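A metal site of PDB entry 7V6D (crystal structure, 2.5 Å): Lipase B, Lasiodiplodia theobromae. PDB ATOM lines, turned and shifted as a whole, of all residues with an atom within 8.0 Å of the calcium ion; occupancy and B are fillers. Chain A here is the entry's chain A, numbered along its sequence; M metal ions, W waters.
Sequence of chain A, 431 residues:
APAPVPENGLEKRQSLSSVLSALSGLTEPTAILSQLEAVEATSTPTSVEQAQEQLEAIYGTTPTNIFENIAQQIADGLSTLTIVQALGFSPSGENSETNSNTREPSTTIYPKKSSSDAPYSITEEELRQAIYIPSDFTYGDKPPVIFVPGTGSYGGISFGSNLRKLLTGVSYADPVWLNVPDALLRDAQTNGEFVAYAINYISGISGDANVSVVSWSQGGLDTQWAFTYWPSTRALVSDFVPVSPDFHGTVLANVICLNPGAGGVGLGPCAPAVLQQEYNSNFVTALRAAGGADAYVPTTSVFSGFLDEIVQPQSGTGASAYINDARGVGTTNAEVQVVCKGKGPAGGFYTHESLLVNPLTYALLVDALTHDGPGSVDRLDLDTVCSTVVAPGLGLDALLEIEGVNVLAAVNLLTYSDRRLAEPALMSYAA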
ATOM      1  N   SER A 212     -11.994 -10.715 -33.749  1.00  0.00           N
ATOM      2  CA  SER A 212     -12.836  -9.609 -33.335  1.00  0.00           C
ATOM      3  C   SER A 212     -12.151  -8.296 -33.707  1.00  0.00           C
ATOM      4  O   SER A 212     -10.931  -8.238 -33.863  1.00  0.00           O
ATOM      5  CB  SER A 212     -13.095  -9.625 -31.834  1.00  0.00           C
ATOM      6  OG  SER A 212     -14.158 -10.496 -31.535  1.00  0.00           O
ATOM      7  N   VAL A 237     -15.693 -12.481 -38.341  1.00  0.00           N
ATOM      8  CA  VAL A 237     -15.688 -11.542 -37.223  1.00  0.00           C
ATOM      9  C   VAL A 237     -16.806 -11.918 -36.266  1.00  0.00           C
ATOM     10  O   VAL A 237     -17.995 -11.741 -36.569  1.00  0.00           O
ATOM     11  CB  VAL A 237     -15.848 -10.085 -37.696  1.00  0.00           C
ATOM     12  CG1 VAL A 237     -15.935  -9.126 -36.494  1.00  0.00           C
ATOM     13  CG2 VAL A 237     -14.734  -9.690 -38.647  1.00  0.00           C
ATOM     14  N   SER A 238     -16.434 -12.416 -35.078  1.00  0.00           N
ATOM     15  CA  SER A 238     -17.443 -12.677 -34.056  1.00  0.00           C
ATOM     16  C   SER A 238     -17.978 -11.370 -33.479  1.00  0.00           C
ATOM     17  O   SER A 238     -19.193 -11.194 -33.349  1.00  0.00           O
ATOM     18  CB  SER A 238     -16.875 -13.574 -32.946  1.00  0.00           C
ATOM     19  OG  SER A 238     -16.365 -14.781 -33.452  1.00  0.00           O
ATOM     20  N   ASP A 239     -17.092 -10.437 -33.134  1.00  0.00           N
ATOM     21  CA  ASP A 239     -17.524  -9.201 -32.516  1.00  0.00           C
ATOM     22  C   ASP A 239     -16.838  -7.986 -33.138  1.00  0.00           C
ATOM     23  O   ASP A 239     -15.614  -7.984 -33.380  1.00  0.00           O
ATOM     24  CB  ASP A 239     -17.292  -9.242 -31.008  1.00  0.00           C
ATOM     25  CG  ASP A 239     -18.260 -10.184 -30.326  1.00  0.00           C
ATOM     26  OD1 ASP A 239     -19.405  -9.759 -30.011  1.00  0.00           O
ATOM     27  OD2 ASP A 239     -17.893 -11.370 -30.142  1.00  0.00           O
ATOM     28  N   PHE A 240     -17.648  -6.969 -33.425  1.00  0.00           N
ATOM     29  CA  PHE A 240     -17.230  -5.636 -33.806  1.00  0.00           C
ATOM     30  C   PHE A 240     -17.630  -4.726 -32.649  1.00  0.00           C
ATOM     31  O   PHE A 240     -18.820  -4.647 -32.314  1.00  0.00           O
ATOM     32  CB  PHE A 240     -17.905  -5.244 -35.118  1.00  0.00           C
ATOM     33  CG  PHE A 240     -17.681  -3.816 -35.528  1.00  0.00           C
ATOM     34  CD1 PHE A 240     -16.502  -3.144 -35.211  1.00  0.00           C
ATOM     35  CD2 PHE A 240     -18.644  -3.150 -36.279  1.00  0.00           C
ATOM     36  CE1 PHE A 240     -16.299  -1.813 -35.601  1.00  0.00           C
ATOM     37  CE2 PHE A 240     -18.440  -1.823 -36.685  1.00  0.00           C
ATOM     38  CZ  PHE A 240     -17.267  -1.159 -36.348  1.00  0.00           C
ATOM     39  N   VAL A 241     -16.640  -4.084 -32.023  1.00  0.00           N
ATOM     40  CA  VAL A 241     -16.882  -3.222 -30.865  1.00  0.00           C
ATOM     41  C   VAL A 241     -16.357  -1.815 -31.157  1.00  0.00           C
ATOM     42  O   VAL A 241     -15.210  -1.473 -30.829  1.00  0.00           O
ATOM     43  CB  VAL A 241     -16.238  -3.818 -29.598  1.00  0.00           C
ATOM     44  CG1 VAL A 241     -16.676  -3.037 -28.364  1.00  0.00           C
ATOM     45  CG2 VAL A 241     -16.607  -5.315 -29.467  1.00  0.00           C
ATOM     46  N   PRO A 298     -22.302  -9.258 -34.959  1.00  0.00           N
ATOM     47  CA  PRO A 298     -22.734  -8.659 -33.689  1.00  0.00           C
ATOM     48  C   PRO A 298     -21.889  -7.429 -33.356  1.00  0.00           C
ATOM     49  O   PRO A 298     -20.654  -7.498 -33.286  1.00  0.00           O
ATOM     50  CB  PRO A 298     -22.534  -9.792 -32.670  1.00  0.00           C
ATOM     51  CG  PRO A 298     -22.653 -11.044 -33.486  1.00  0.00           C
ATOM     52  CD  PRO A 298     -21.988 -10.689 -34.803  1.00  0.00           C
ATOM     53  N   THR A 299     -22.558  -6.290 -33.174  1.00  0.00           N
ATOM     54  CA  THR A 299     -21.912  -4.994 -33.044  1.00  0.00           C
ATOM     55  C   THR A 299     -22.308  -4.355 -31.717  1.00  0.00           C
ATOM     56  O   THR A 299     -23.497  -4.141 -31.433  1.00  0.00           O
ATOM     57  CB  THR A 299     -22.302  -4.081 -34.205  1.00  0.00           C
ATOM     58  OG1 THR A 299     -21.853  -4.664 -35.448  1.00  0.00           O
ATOM     59  CG2 THR A 299     -21.647  -2.713 -34.029  1.00  0.00           C
ATOM     60  N   THR A 300     -21.301  -4.026 -30.912  1.00  0.00           N
ATOM     61  CA  THR A 300     -21.484  -3.368 -29.630  1.00  0.00           C
ATOM     62  C   THR A 300     -20.938  -1.940 -29.781  1.00  0.00           C
ATOM     63  O   THR A 300     -19.742  -1.698 -29.607  1.00  0.00           O
ATOM     64  CB  THR A 300     -20.759  -4.128 -28.531  1.00  0.00           C
ATOM     65  OG1 THR A 300     -21.097  -5.519 -28.604  1.00  0.00           O
ATOM     66  CG2 THR A 300     -21.112  -3.536 -27.169  1.00  0.00           C
ATOM     67  N   LEU A 364     -18.658  -3.727 -21.464  1.00  0.00           N
ATOM     68  CA  LEU A 364     -19.369  -4.185 -22.655  1.00  0.00           C
ATOM     69  C   LEU A 364     -18.441  -4.894 -23.632  1.00  0.00           C
ATOM     70  O   LEU A 364     -18.891  -5.747 -24.403  1.00  0.00           O
ATOM     71  CB  LEU A 364     -20.037  -3.004 -23.354  1.00  0.00           C
ATOM     72  CG  LEU A 364     -21.394  -2.589 -22.835  1.00  0.00           C
ATOM     73  CD1 LEU A 364     -21.762  -1.275 -23.491  1.00  0.00           C
ATOM     74  CD2 LEU A 364     -22.438  -3.708 -23.089  1.00  0.00           C
ATOM     75  N   LEU A 365     -17.149  -4.551 -23.614  1.00  0.00           N
ATOM     76  CA  LEU A 365     -16.209  -5.215 -24.495  1.00  0.00           C
ATOM     77  C   LEU A 365     -15.991  -6.669 -24.068  1.00  0.00           C
ATOM     78  O   LEU A 365     -16.015  -7.579 -24.899  1.00  0.00           O
ATOM     79  CB  LEU A 365     -14.896  -4.427 -24.515  1.00  0.00           C
ATOM     80  CG  LEU A 365     -13.694  -5.051 -25.226  1.00  0.00           C
ATOM     81  CD1 LEU A 365     -13.962  -5.235 -26.718  1.00  0.00           C
ATOM     82  CD2 LEU A 365     -12.495  -4.175 -24.998  1.00  0.00           C
ATOM     83  N   VAL A 366     -15.775  -6.887 -22.774  1.00  0.00           N
ATOM     84  CA  VAL A 366     -15.493  -8.219 -22.264  1.00  0.00           C
ATOM     85  C   VAL A 366     -16.723  -9.099 -22.403  1.00  0.00           C
ATOM     86  O   VAL A 366     -16.637 -10.263 -22.838  1.00  0.00           O
ATOM     87  CB  VAL A 366     -15.045  -8.124 -20.799  1.00  0.00           C
ATOM     88  CG1 VAL A 366     -14.914  -9.521 -20.171  1.00  0.00           C
ATOM     89  CG2 VAL A 366     -13.757  -7.336 -20.676  1.00  0.00           C
ATOM     90  N   ASP A 367     -17.888  -8.557 -22.034  1.00  0.00           N
ATOM     91  CA  ASP A 367     -19.142  -9.279 -22.209  1.00  0.00           C
ATOM     92  C   ASP A 367     -19.293  -9.748 -23.651  1.00  0.00           C
ATOM     93  O   ASP A 367     -19.613 -10.917 -23.897  1.00  0.00           O
ATOM     94  CB  ASP A 367     -20.308  -8.387 -21.798  1.00  0.00           C
ATOM     95  CG  ASP A 367     -21.610  -9.163 -21.714  1.00  0.00           C
ATOM     96  OD1 ASP A 367     -21.853  -9.825 -20.668  1.00  0.00           O
ATOM     97  OD2 ASP A 367     -22.383  -9.101 -22.701  1.00  0.00           O
ATOM     98  N   ALA A 368     -19.039  -8.865 -24.617  1.00  0.00           N
ATOM     99  CA  ALA A 368     -19.175  -9.215 -26.026  1.00  0.00           C
ATOM    100  C   ALA A 368     -18.211 -10.322 -26.407  1.00  0.00           C
ATOM    101  O   ALA A 368     -18.519 -11.155 -27.264  1.00  0.00           O
ATOM    102  CB  ALA A 368     -18.919  -7.996 -26.910  1.00  0.00           C
ATOM    103  N   LEU A 369     -17.022 -10.329 -25.816  1.00  0.00           N
ATOM    104  CA  LEU A 369     -16.014 -11.308 -26.207  1.00  0.00           C
ATOM    105  C   LEU A 369     -16.242 -12.660 -25.548  1.00  0.00           C
ATOM    106  O   LEU A 369     -15.715 -13.665 -26.039  1.00  0.00           O
ATOM    107  CB  LEU A 369     -14.610 -10.790 -25.858  1.00  0.00           C
ATOM    108  CG  LEU A 369     -14.137  -9.560 -26.632  1.00  0.00           C
ATOM    109  CD1 LEU A 369     -12.674  -9.256 -26.348  1.00  0.00           C
ATOM    110  CD2 LEU A 369     -14.372  -9.771 -28.120  1.00  0.00           C
ATOM    111  N   THR A 370     -17.008 -12.706 -24.468  1.00  0.00           N
ATOM    112  CA  THR A 370     -17.195 -13.928 -23.699  1.00  0.00           C
ATOM    113  C   THR A 370     -18.606 -14.524 -23.851  1.00  0.00           C
ATOM    114  O   THR A 370     -19.007 -15.367 -23.046  1.00  0.00           O
ATOM    115  CB  THR A 370     -16.861 -13.665 -22.219  1.00  0.00           C
ATOM    116  OG1 THR A 370     -17.621 -12.544 -21.743  1.00  0.00           O
ATOM    117  CG2 THR A 370     -15.378 -13.334 -22.068  1.00  0.00           C
ATOM    118  N   HIS A 371     -19.359 -14.095 -24.872  1.00  0.00           N
ATOM    119  CA  HIS A 371     -20.740 -14.515 -25.085  1.00  0.00           C
ATOM    120  C   HIS A 371     -21.100 -14.398 -26.565  1.00  0.00           C
ATOM    121  O   HIS A 371     -20.717 -13.429 -27.214  1.00  0.00           O
ATOM    122  CB  HIS A 371     -21.724 -13.655 -24.302  1.00  0.00           C
ATOM    123  CG  HIS A 371     -21.513 -13.688 -22.828  1.00  0.00           C
ATOM    124  ND1 HIS A 371     -20.567 -12.907 -22.192  1.00  0.00           N
ATOM    125  CD2 HIS A 371     -22.108 -14.416 -21.861  1.00  0.00           C
ATOM    126  CE1 HIS A 371     -20.596 -13.158 -20.895  1.00  0.00           C
ATOM    127  NE2 HIS A 371     -21.531 -14.059 -20.662  1.00  0.00           N
ATOM    128  N   ASP A 372     -21.876 -15.364 -27.073  1.00  0.00           N
ATOM    129  CA  ASP A 372     -22.464 -15.191 -28.393  1.00  0.00           C
ATOM    130  C   ASP A 372     -23.222 -13.872 -28.440  1.00  0.00           C
ATOM    131  O   ASP A 372     -23.850 -13.470 -27.446  1.00  0.00           O
ATOM    132  CB  ASP A 372     -23.414 -16.345 -28.751  1.00  0.00           C
ATOM    133  CG  ASP A 372     -22.717 -17.714 -28.838  1.00  0.00           C
ATOM    134  OD1 ASP A 372     -21.476 -17.787 -28.688  1.00  0.00           O
ATOM    135  OD2 ASP A 372     -23.429 -18.719 -29.071  1.00  0.00           O
ATOM    136  N   GLY A 373     -23.165 -13.199 -29.582  1.00  0.00           N
ATOM    137  CA  GLY A 373     -23.845 -11.939 -29.762  1.00  0.00           C
ATOM    138  C   GLY A 373     -23.065 -10.787 -29.169  1.00  0.00           C
ATOM    139  O   GLY A 373     -21.912 -10.939 -28.768  1.00  0.00           O
ATOM    140  N   PRO A 374     -23.681  -9.612 -29.097  1.00  0.00           N
ATOM    141  CA  PRO A 374     -22.955  -8.416 -28.660  1.00  0.00           C
ATOM    142  C   PRO A 374     -22.904  -8.311 -27.142  1.00  0.00           C
ATOM    143  O   PRO A 374     -23.476  -9.098 -26.397  1.00  0.00           O
ATOM    144  CB  PRO A 374     -23.775  -7.278 -29.279  1.00  0.00           C
ATOM    145  CG  PRO A 374     -25.185  -7.824 -29.265  1.00  0.00           C
ATOM    146  CD  PRO A 374     -25.047  -9.285 -29.554  1.00  0.00           C
ATOM    147  N   GLY A 375     -22.179  -7.287 -26.673  1.00  0.00           N
ATOM    148  CA  GLY A 375     -22.221  -6.990 -25.261  1.00  0.00           C
ATOM    149  C   GLY A 375     -23.625  -6.622 -24.845  1.00  0.00           C
ATOM    150  O   GLY A 375     -24.355  -5.934 -25.573  1.00  0.00           O
ATOM    151  N   ARG A 379     -27.301  -7.858 -19.086  1.00  0.00           N
ATOM    152  CA  ARG A 379     -26.571  -8.895 -18.370  1.00  0.00           C
ATOM    153  C   ARG A 379     -25.547  -8.295 -17.409  1.00  0.00           C
ATOM    154  O   ARG A 379     -25.156  -8.957 -16.455  1.00  0.00           O
ATOM    155  CB  ARG A 379     -25.890  -9.840 -19.375  1.00  0.00           C
ATOM    156  CG  ARG A 379     -24.917 -10.853 -18.763  1.00  0.00           C
ATOM    157  CD  ARG A 379     -24.459 -11.925 -19.758  1.00  0.00           C
ATOM    158  NE  ARG A 379     -24.067 -11.398 -21.055  1.00  0.00           N
ATOM    159  CZ  ARG A 379     -24.342 -11.985 -22.212  1.00  0.00           C
ATOM    160  NH1 ARG A 379     -24.971 -13.138 -22.250  1.00  0.00           N
ATOM    161  NH2 ARG A 379     -23.997 -11.373 -23.345  1.00  0.00           N
HETATM  162 CA    CA M   1     -19.854 -12.072 -28.897  1.00  0.00          CA
HETATM  163  O   HOH W   1     -20.621 -12.372 -31.152  1.00  0.00           O
HETATM  164  O   HOH W   2     -18.364 -14.191 -28.898  1.00  0.00           O
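Water W1 lies within hydrogen-bond range of O of Ser 238 (2.9 Å) and N of Gly 373 (3.1 Å).
Merely in contact with the calcium ion: Asp 372 (3.8 Å).
Of the 22 residues printed, 5 come within 4 Å of the calcium ion.
The calcium ion is bound by O of Ala 368 (2.3 Å), O of His 371 (2.3 Å), O of Gly 373 (2.4 Å), water W1 (2.4 Å), OD2 of Asp 239 (2.4 Å), water W2 (2.6 Å) and OD1 of Asp 239 (2.6 Å).
The backbone NH (N) of Asp 239 sits at hydrogen-bond distance from the side-chain hydroxyl (OG) of Ser 212, 3.3 Å away.
A ring nitrogen (ND1) of His 371 lies within hydrogen-bond range of the side-chain hydroxyl of Thr 370 (3.0 Å).
A ring nitrogen (ND1) of His 371 lies within hydrogen-bond range of the backbone carbonyl oxygen (O) of Asp 367, at 2.8 Å.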
